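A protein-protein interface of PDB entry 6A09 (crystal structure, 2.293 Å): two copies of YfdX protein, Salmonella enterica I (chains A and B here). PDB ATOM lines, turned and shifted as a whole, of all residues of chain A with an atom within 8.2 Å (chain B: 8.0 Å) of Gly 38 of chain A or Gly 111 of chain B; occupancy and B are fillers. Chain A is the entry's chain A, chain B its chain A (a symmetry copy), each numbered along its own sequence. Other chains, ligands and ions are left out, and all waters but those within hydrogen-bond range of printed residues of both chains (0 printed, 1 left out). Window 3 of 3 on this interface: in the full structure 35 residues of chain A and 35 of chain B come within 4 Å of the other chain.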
ATOM      1  N   SER A  31      -0.683 -19.164 -18.105  1.00  0.00           N
ATOM      2  CA  SER A  31      -0.327 -19.630 -19.439  1.00  0.00           C
ATOM      3  C   SER A  31       1.034 -20.317 -19.438  1.00  0.00           C
ATOM      4  O   SER A  31       1.183 -21.421 -19.967  1.00  0.00           O
ATOM      5  CB  SER A  31      -0.342 -18.452 -20.416  1.00  0.00           C
ATOM      6  OG  SER A  31       0.195 -18.828 -21.672  1.00  0.00           O
ATOM      7  N   ARG A  32       2.044 -19.672 -18.850  1.00  0.00           N
ATOM      8  CA  ARG A  32       3.363 -20.291 -18.770  1.00  0.00           C
ATOM      9  C   ARG A  32       3.297 -21.635 -18.057  1.00  0.00           C
ATOM     10  O   ARG A  32       3.930 -22.608 -18.497  1.00  0.00           O
ATOM     11  CB  ARG A  32       4.339 -19.358 -18.057  1.00  0.00           C
ATOM     12  CG  ARG A  32       5.768 -19.860 -18.019  1.00  0.00           C
ATOM     13  CD  ARG A  32       6.686 -18.714 -17.621  1.00  0.00           C
ATOM     14  NE  ARG A  32       8.063 -19.147 -17.415  1.00  0.00           N
ATOM     15  CZ  ARG A  32       8.529 -19.608 -16.255  1.00  0.00           C
ATOM     16  NH1 ARG A  32       7.718 -19.703 -15.207  1.00  0.00           N
ATOM     17  NH2 ARG A  32       9.803 -19.979 -16.142  1.00  0.00           N
ATOM     18  N   PHE A  33       2.517 -21.724 -16.966  1.00  0.00           N
ATOM     19  CA  PHE A  33       2.439 -22.999 -16.277  1.00  0.00           C
ATOM     20  C   PHE A  33       1.870 -24.090 -17.179  1.00  0.00           C
ATOM     21  O   PHE A  33       2.379 -25.219 -17.194  1.00  0.00           O
ATOM     22  CB  PHE A  33       1.614 -22.911 -14.998  1.00  0.00           C
ATOM     23  CG  PHE A  33       1.450 -24.242 -14.343  1.00  0.00           C
ATOM     24  CD1 PHE A  33       2.455 -24.748 -13.535  1.00  0.00           C
ATOM     25  CD2 PHE A  33       0.345 -25.045 -14.620  1.00  0.00           C
ATOM     26  CE1 PHE A  33       2.330 -26.020 -12.951  1.00  0.00           C
ATOM     27  CE2 PHE A  33       0.223 -26.309 -14.058  1.00  0.00           C
ATOM     28  CZ  PHE A  33       1.222 -26.798 -13.215  1.00  0.00           C
ATOM     29  N   GLU A  34       0.797 -23.785 -17.917  1.00  0.00           N
ATOM     30  CA  GLU A  34       0.152 -24.806 -18.732  1.00  0.00           C
ATOM     31  C   GLU A  34       1.055 -25.294 -19.863  1.00  0.00           C
ATOM     32  O   GLU A  34       0.912 -26.445 -20.306  1.00  0.00           O
ATOM     33  CB  GLU A  34      -1.170 -24.271 -19.289  1.00  0.00           C
ATOM     34  CG  GLU A  34      -2.222 -23.966 -18.224  1.00  0.00           C
ATOM     35  CD  GLU A  34      -2.630 -25.193 -17.362  1.00  0.00           C
ATOM     36  OE1 GLU A  34      -2.303 -26.349 -17.708  1.00  0.00           O
ATOM     37  OE2 GLU A  34      -3.308 -24.996 -16.334  1.00  0.00           O
ATOM     38  N   LEU A  35       1.966 -24.440 -20.353  1.00  0.00           N
ATOM     39  CA  LEU A  35       2.988 -24.892 -21.298  1.00  0.00           C
ATOM     40  C   LEU A  35       3.725 -26.127 -20.771  1.00  0.00           C
ATOM     41  O   LEU A  35       3.762 -27.189 -21.411  1.00  0.00           O
ATOM     42  CB  LEU A  35       3.976 -23.752 -21.568  1.00  0.00           C
ATOM     43  CG  LEU A  35       3.444 -22.538 -22.338  1.00  0.00           C
ATOM     44  CD1 LEU A  35       4.523 -21.440 -22.495  1.00  0.00           C
ATOM     45  CD2 LEU A  35       2.909 -22.960 -23.707  1.00  0.00           C
ATOM     46  N   PHE A  36       4.317 -26.003 -19.585  1.00  0.00           N
ATOM     47  CA  PHE A  36       5.015 -27.139 -19.009  1.00  0.00           C
ATOM     48  C   PHE A  36       4.062 -28.251 -18.595  1.00  0.00           C
ATOM     49  O   PHE A  36       4.486 -29.401 -18.486  1.00  0.00           O
ATOM     50  CB  PHE A  36       5.848 -26.684 -17.823  1.00  0.00           C
ATOM     51  CG  PHE A  36       6.943 -25.737 -18.190  1.00  0.00           C
ATOM     52  CD1 PHE A  36       8.211 -26.208 -18.499  1.00  0.00           C
ATOM     53  CD2 PHE A  36       6.721 -24.371 -18.200  1.00  0.00           C
ATOM     54  CE1 PHE A  36       9.235 -25.340 -18.810  1.00  0.00           C
ATOM     55  CE2 PHE A  36       7.746 -23.492 -18.525  1.00  0.00           C
ATOM     56  CZ  PHE A  36       9.010 -23.985 -18.832  1.00  0.00           C
ATOM     57  N   ASN A  37       2.789 -27.942 -18.386  1.00  0.00           N
ATOM     58  CA  ASN A  37       1.814 -28.938 -17.966  1.00  0.00           C
ATOM     59  C   ASN A  37       1.297 -29.760 -19.133  1.00  0.00           C
ATOM     60  O   ASN A  37       0.398 -30.584 -18.940  1.00  0.00           O
ATOM     61  CB  ASN A  37       0.644 -28.260 -17.244  1.00  0.00           C
ATOM     62  CG  ASN A  37      -0.065 -29.188 -16.259  1.00  0.00           C
ATOM     63  OD1 ASN A  37       0.544 -30.110 -15.719  1.00  0.00           O
ATOM     64  ND2 ASN A  37      -1.354 -28.928 -16.006  1.00  0.00           N
ATOM     65  N   GLY A  38       1.844 -29.547 -20.329  1.00  0.00           N
ATOM     66  CA  GLY A  38       1.399 -30.271 -21.503  1.00  0.00           C
ATOM     67  C   GLY A  38      -0.005 -29.929 -21.951  1.00  0.00           C
ATOM     68  O   GLY A  38      -0.688 -30.789 -22.521  1.00  0.00           O
ATOM     69  N   ARG A  39      -0.459 -28.683 -21.710  1.00  0.00           N
ATOM     70  CA  ARG A  39      -1.761 -28.202 -22.185  1.00  0.00           C
ATOM     71  C   ARG A  39      -1.555 -26.909 -22.991  1.00  0.00           C
ATOM     72  O   ARG A  39      -2.013 -25.825 -22.612  1.00  0.00           O
ATOM     73  CB  ARG A  39      -2.732 -28.018 -21.017  1.00  0.00           C
ATOM     74  CG  ARG A  39      -3.009 -29.357 -20.331  1.00  0.00           C
ATOM     75  CD  ARG A  39      -4.320 -29.402 -19.602  1.00  0.00           C
ATOM     76  NE  ARG A  39      -4.325 -28.470 -18.480  1.00  0.00           N
ATOM     77  CZ  ARG A  39      -5.140 -28.568 -17.432  1.00  0.00           C
ATOM     78  NH1 ARG A  39      -5.992 -29.579 -17.357  1.00  0.00           N
ATOM     79  NH2 ARG A  39      -5.088 -27.670 -16.452  1.00  0.00           N
ATOM     80  N   THR A  40      -0.878 -27.054 -24.137  1.00  0.00           N
ATOM     81  CA  THR A  40      -0.487 -25.901 -24.948  1.00  0.00           C
ATOM     82  C   THR A  40      -1.701 -25.140 -25.468  1.00  0.00           C
ATOM     83  O   THR A  40      -1.683 -23.905 -25.546  1.00  0.00           O
ATOM     84  CB  THR A  40       0.398 -26.358 -26.110  1.00  0.00           C
ATOM     85  OG1 THR A  40      -0.259 -27.418 -26.822  1.00  0.00           O
ATOM     86  CG2 THR A  40       1.747 -26.856 -25.587  1.00  0.00           C
ATOM     87  N   GLN A  41      -2.763 -25.856 -25.816  1.00  0.00           N
ATOM     88  CA  GLN A  41      -3.988 -25.204 -26.268  1.00  0.00           C
ATOM     89  C   GLN A  41      -4.580 -24.304 -25.186  1.00  0.00           C
ATOM     90  O   GLN A  41      -5.028 -23.188 -25.471  1.00  0.00           O
ATOM     91  CB  GLN A  41      -4.992 -26.265 -26.703  1.00  0.00           C
ATOM     92  CG  GLN A  41      -6.224 -25.704 -27.352  1.00  0.00           C
ATOM     93  CD  GLN A  41      -6.942 -26.735 -28.196  1.00  0.00           C
ATOM     94  OE1 GLN A  41      -6.363 -27.289 -29.141  1.00  0.00           O
ATOM     95  NE2 GLN A  41      -8.211 -26.999 -27.870  1.00  0.00           N
ATOM     96  N   LYS A  42      -4.605 -24.777 -23.940  1.00  0.00           N
ATOM     97  CA  LYS A  42      -5.049 -23.935 -22.830  1.00  0.00           C
ATOM     98  C   LYS A  42      -4.073 -22.795 -22.580  1.00  0.00           C
ATOM     99  O   LYS A  42      -4.480 -21.681 -22.234  1.00  0.00           O
ATOM    100  CB  LYS A  42      -5.212 -24.789 -21.565  1.00  0.00           C
ATOM    101  CG  LYS A  42      -5.681 -24.060 -20.313  1.00  0.00           C
ATOM    102  CD  LYS A  42      -6.015 -25.092 -19.220  1.00  0.00           C
ATOM    103  CE  LYS A  42      -6.053 -24.485 -17.810  1.00  0.00           C
ATOM    104  NZ  LYS A  42      -7.462 -24.200 -17.357  1.00  0.00           N
ATOM    105  N   ALA A  43      -2.781 -23.059 -22.745  1.00  0.00           N
ATOM    106  CA  ALA A  43      -1.792 -22.000 -22.639  1.00  0.00           C
ATOM    107  C   ALA A  43      -2.051 -20.884 -23.654  1.00  0.00           C
ATOM    108  O   ALA A  43      -1.977 -19.706 -23.303  1.00  0.00           O
ATOM    109  CB  ALA A  43      -0.397 -22.590 -22.804  1.00  0.00           C
ATOM    110  N   LEU B  12       1.783 -30.456 -11.758  1.00  0.00           N
ATOM    111  CA  LEU B  12       2.376 -31.370 -12.734  1.00  0.00           C
ATOM    112  C   LEU B  12       2.065 -32.830 -12.411  1.00  0.00           C
ATOM    113  O   LEU B  12       1.874 -33.639 -13.328  1.00  0.00           O
ATOM    114  CB  LEU B  12       3.887 -31.159 -12.818  1.00  0.00           C
ATOM    115  CG  LEU B  12       4.343 -29.824 -13.412  1.00  0.00           C
ATOM    116  CD1 LEU B  12       5.862 -29.773 -13.482  1.00  0.00           C
ATOM    117  CD2 LEU B  12       3.732 -29.596 -14.793  1.00  0.00           C
ATOM    118  N   ALA B 104      11.611 -31.167 -26.658  1.00  0.00           N
ATOM    119  CA  ALA B 104      10.752 -30.821 -25.522  1.00  0.00           C
ATOM    120  C   ALA B 104       9.479 -30.112 -25.984  1.00  0.00           C
ATOM    121  O   ALA B 104       8.402 -30.338 -25.422  1.00  0.00           O
ATOM    122  CB  ALA B 104      11.525 -29.964 -24.510  1.00  0.00           C
ATOM    123  N   ASN B 105       9.579 -29.271 -27.023  1.00  0.00           N
ATOM    124  CA  ASN B 105       8.387 -28.627 -27.574  1.00  0.00           C
ATOM    125  C   ASN B 105       7.407 -29.650 -28.141  1.00  0.00           C
ATOM    126  O   ASN B 105       6.185 -29.497 -28.000  1.00  0.00           O
ATOM    127  CB  ASN B 105       8.783 -27.610 -28.652  1.00  0.00           C
ATOM    128  CG  ASN B 105       9.379 -26.354 -28.063  1.00  0.00           C
ATOM    129  OD1 ASN B 105       9.175 -26.048 -26.886  1.00  0.00           O
ATOM    130  ND2 ASN B 105      10.110 -25.610 -28.875  1.00  0.00           N
ATOM    131  N   GLN B 106       7.921 -30.690 -28.805  1.00  0.00           N
ATOM    132  CA  GLN B 106       7.030 -31.715 -29.341  1.00  0.00           C
ATOM    133  C   GLN B 106       6.331 -32.467 -28.212  1.00  0.00           C
ATOM    134  O   GLN B 106       5.128 -32.746 -28.292  1.00  0.00           O
ATOM    135  CB  GLN B 106       7.815 -32.672 -30.240  1.00  0.00           C
ATOM    136  CG  GLN B 106       6.957 -33.733 -30.928  1.00  0.00           C
ATOM    137  CD  GLN B 106       5.905 -33.120 -31.828  1.00  0.00           C
ATOM    138  OE1 GLN B 106       6.189 -32.181 -32.581  1.00  0.00           O
ATOM    139  NE2 GLN B 106       4.677 -33.637 -31.749  1.00  0.00           N
ATOM    140  N   LYS B 107       7.065 -32.770 -27.135  1.00  0.00           N
ATOM    141  CA  LYS B 107       6.471 -33.444 -25.980  1.00  0.00           C
ATOM    142  C   LYS B 107       5.377 -32.601 -25.322  1.00  0.00           C
ATOM    143  O   LYS B 107       4.367 -33.146 -24.858  1.00  0.00           O
ATOM    144  CB  LYS B 107       7.558 -33.794 -24.970  1.00  0.00           C
ATOM    145  CG  LYS B 107       8.606 -34.713 -25.528  1.00  0.00           C
ATOM    146  CD  LYS B 107       7.971 -36.022 -25.931  1.00  0.00           C
ATOM    147  CE  LYS B 107       9.025 -37.031 -26.371  1.00  0.00           C
ATOM    148  NZ  LYS B 107       8.419 -38.381 -26.547  1.00  0.00           N
ATOM    149  N   MET B 108       5.551 -31.272 -25.281  1.00  0.00           N
ATOM    150  CA  MET B 108       4.502 -30.417 -24.724  1.00  0.00           C
ATOM    151  C   MET B 108       3.257 -30.422 -25.606  1.00  0.00           C
ATOM    152  O   MET B 108       2.128 -30.496 -25.092  1.00  0.00           O
ATOM    153  CB  MET B 108       5.020 -28.985 -24.526  1.00  0.00           C
ATOM    154  CG  MET B 108       5.919 -28.805 -23.302  1.00  0.00           C
ATOM    155  SD  MET B 108       6.678 -27.162 -23.154  1.00  0.00           S
ATOM    156  CE  MET B 108       8.286 -27.467 -23.833  1.00  0.00           C
ATOM    157  N   LYS B 109       3.441 -30.321 -26.933  1.00  0.00           N
ATOM    158  CA  LYS B 109       2.320 -30.477 -27.862  1.00  0.00           C
ATOM    159  C   LYS B 109       1.598 -31.791 -27.610  1.00  0.00           C
ATOM    160  O   LYS B 109       0.366 -31.835 -27.557  1.00  0.00           O
ATOM    161  CB  LYS B 109       2.810 -30.425 -29.320  1.00  0.00           C
ATOM    162  CG  LYS B 109       1.848 -29.811 -30.339  1.00  0.00           C
ATOM    163  CD  LYS B 109       0.465 -30.369 -30.243  1.00  0.00           C
ATOM    164  CE  LYS B 109      -0.530 -29.643 -30.984  1.00  0.00           C
ATOM    165  NZ  LYS B 109      -1.881 -29.958 -30.495  1.00  0.00           N
ATOM    166  N   GLU B 110       2.353 -32.870 -27.429  1.00  0.00           N
ATOM    167  CA  GLU B 110       1.765 -34.184 -27.224  1.00  0.00           C
ATOM    168  C   GLU B 110       1.134 -34.346 -25.846  1.00  0.00           C
ATOM    169  O   GLU B 110       0.496 -35.377 -25.592  1.00  0.00           O
ATOM    170  CB  GLU B 110       2.841 -35.249 -27.471  1.00  0.00           C
ATOM    171  CG  GLU B 110       3.184 -35.370 -28.954  1.00  0.00           C
ATOM    172  CD  GLU B 110       4.540 -36.009 -29.231  1.00  0.00           C
ATOM    173  OE1 GLU B 110       5.271 -36.358 -28.278  1.00  0.00           O
ATOM    174  OE2 GLU B 110       4.881 -36.159 -30.425  1.00  0.00           O
ATOM    175  N   GLY B 111       1.272 -33.363 -24.961  1.00  0.00           N
ATOM    176  CA  GLY B 111       0.739 -33.528 -23.626  1.00  0.00           C
ATOM    177  C   GLY B 111       1.496 -34.523 -22.782  1.00  0.00           C
ATOM    178  O   GLY B 111       0.956 -35.021 -21.798  1.00  0.00           O
ATOM    179  N   ASP B 112       2.751 -34.799 -23.130  1.00  0.00           N
ATOM    180  CA  ASP B 112       3.583 -35.821 -22.491  1.00  0.00           C
ATOM    181  C   ASP B 112       4.446 -35.132 -21.440  1.00  0.00           C
ATOM    182  O   ASP B 112       5.557 -34.690 -21.730  1.00  0.00           O
ATOM    183  CB  ASP B 112       4.434 -36.525 -23.551  1.00  0.00           C
ATOM    184  CG  ASP B 112       5.381 -37.584 -22.965  1.00  0.00           C
ATOM    185  OD1 ASP B 112       5.421 -37.757 -21.731  1.00  0.00           O
ATOM    186  OD2 ASP B 112       6.102 -38.242 -23.757  1.00  0.00           O
ATOM    187  N   LYS B 113       3.942 -35.068 -20.204  1.00  0.00           N
ATOM    188  CA  LYS B 113       4.638 -34.335 -19.145  1.00  0.00           C
ATOM    189  C   LYS B 113       5.996 -34.955 -18.832  1.00  0.00           C
ATOM    190  O   LYS B 113       7.001 -34.241 -18.712  1.00  0.00           O
ATOM    191  CB  LYS B 113       3.771 -34.268 -17.884  1.00  0.00           C
ATOM    192  CG  LYS B 113       2.489 -33.465 -18.038  1.00  0.00           C
ATOM    193  CD  LYS B 113       1.844 -33.181 -16.689  1.00  0.00           C
ATOM    194  CE  LYS B 113       0.318 -33.178 -16.787  1.00  0.00           C
ATOM    195  NZ  LYS B 113      -0.426 -32.764 -15.520  1.00  0.00           N
ATOM    196  N   LYS B 114       6.055 -36.286 -18.691  1.00  0.00           N
ATOM    197  CA  LYS B 114       7.338 -36.919 -18.371  1.00  0.00           C
ATOM    198  C   LYS B 114       8.324 -36.804 -19.527  1.00  0.00           C
ATOM    199  O   LYS B 114       9.532 -36.632 -19.302  1.00  0.00           O
ATOM    200  CB  LYS B 114       7.152 -38.388 -17.967  1.00  0.00           C
ATOM    201  CG  LYS B 114       8.457 -39.086 -17.521  1.00  0.00           C
ATOM    202  CD  LYS B 114       9.230 -38.178 -16.535  1.00  0.00           C
ATOM    203  CE  LYS B 114      10.702 -38.563 -16.324  1.00  0.00           C
ATOM    204  NZ  LYS B 114      11.596 -37.375 -16.013  1.00  0.00           N
ATOM    205  N   GLY B 115       7.831 -36.872 -20.771  1.00  0.00           N
ATOM    206  CA  GLY B 115       8.706 -36.640 -21.910  1.00  0.00           C
ATOM    207  C   GLY B 115       9.241 -35.222 -21.938  1.00  0.00           C
ATOM    208  O   GLY B 115      10.401 -34.983 -22.292  1.00  0.00           O
ATOM    209  N   THR B 116       8.415 -34.262 -21.525  1.00  0.00           N
ATOM    210  CA  THR B 116       8.860 -32.880 -21.489  1.00  0.00           C
ATOM    211  C   THR B 116       9.998 -32.692 -20.496  1.00  0.00           C
ATOM    212  O   THR B 116      10.982 -32.011 -20.794  1.00  0.00           O
ATOM    213  CB  THR B 116       7.686 -31.971 -21.149  1.00  0.00           C
ATOM    214  OG1 THR B 116       6.664 -32.138 -22.141  1.00  0.00           O
ATOM    215  CG2 THR B 116       8.150 -30.517 -21.099  1.00  0.00           C
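Phe 33 of chain A touches Leu 12 of chain B (CZ to N, 3.98 Å).
O of Phe 36 of chain A touches CD2 of Leu 12 of chain B (3.8 Å).
CD2 of Leu 12 of chain B touches OD1 of Asn 37 of chain A (3.4 Å).
Met 108 of chain B touches Gly 38 of chain A.
Gly 38 of chain A touches Gly 111 of chain B.
O of Met 108 of chain B touches CG2 of Thr 40 of chain A, at 3.7 Å.
The backbone NH (N) of Met 108 of chain B is in hydrogen-bond range of the side-chain hydroxyl (OG1) of Thr 116 of chain B (3.4 Å).
The side-chain carboxylate (OE1) of Glu 34 of chain A is in hydrogen-bond range of the side-chain amide nitrogen (ND2) of Asn 37 of chain A (3.2 Å).
O of Leu 12 of chain B sits at hydrogen-bond distance from NZ of Lys 113 of chain B (3.3 Å).
Printed residues of chain A that touch a printed residue of chain B: Phe 33, Leu 35, Phe 36, Asn 37, Gly 38 and Thr 40.
Of the 14 printed residues of chain B, 4 touch a printed residue of chain A.
Among the printed residues, 8 pairs touch across the chains.
Among the printed residues, no Asp or Glu carboxylate lies within 4 Å of a Lys or Arg side-chain nitrogen of the other chain.
Gly 38 of chain A touches just these residues of chain B: Met 108 and Gly 111.
Of chain A, only Gly 38 (3.3 Å) comes within 4 Å of Gly 111 of chain B.
Of the printed residues of chain B, Thr 40 of chain A touches Met 108 (3.7 Å).
Of the printed residues of chain B, Asn 37 of chain A touches Leu 12 and Lys 113.
Of the printed residues of chain A, Lys 113 of chain B touches Asn 37 (2.8 Å).
Of the printed residues of chain A, Leu 12 of chain B touches Phe 33 (3.98 Å), Phe 36 (3.8 Å) and Asn 37 (3.4 Å).
Lys 109 of chain B touches none of the printed residues of chain A.
Gly 115 of chain B touches none of the printed residues of chain A.
No position is printed for both chains.
OD1 of Asn 37 of chain A lies within hydrogen-bond range of NZ of Lys 113 of chain B, at 2.8 Å.
The backbone carbonyl oxygen (O) of Leu 35 of chain A sits close to the side-chain sulfur (SD) of Met 108 of chain B (3.4 Å).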
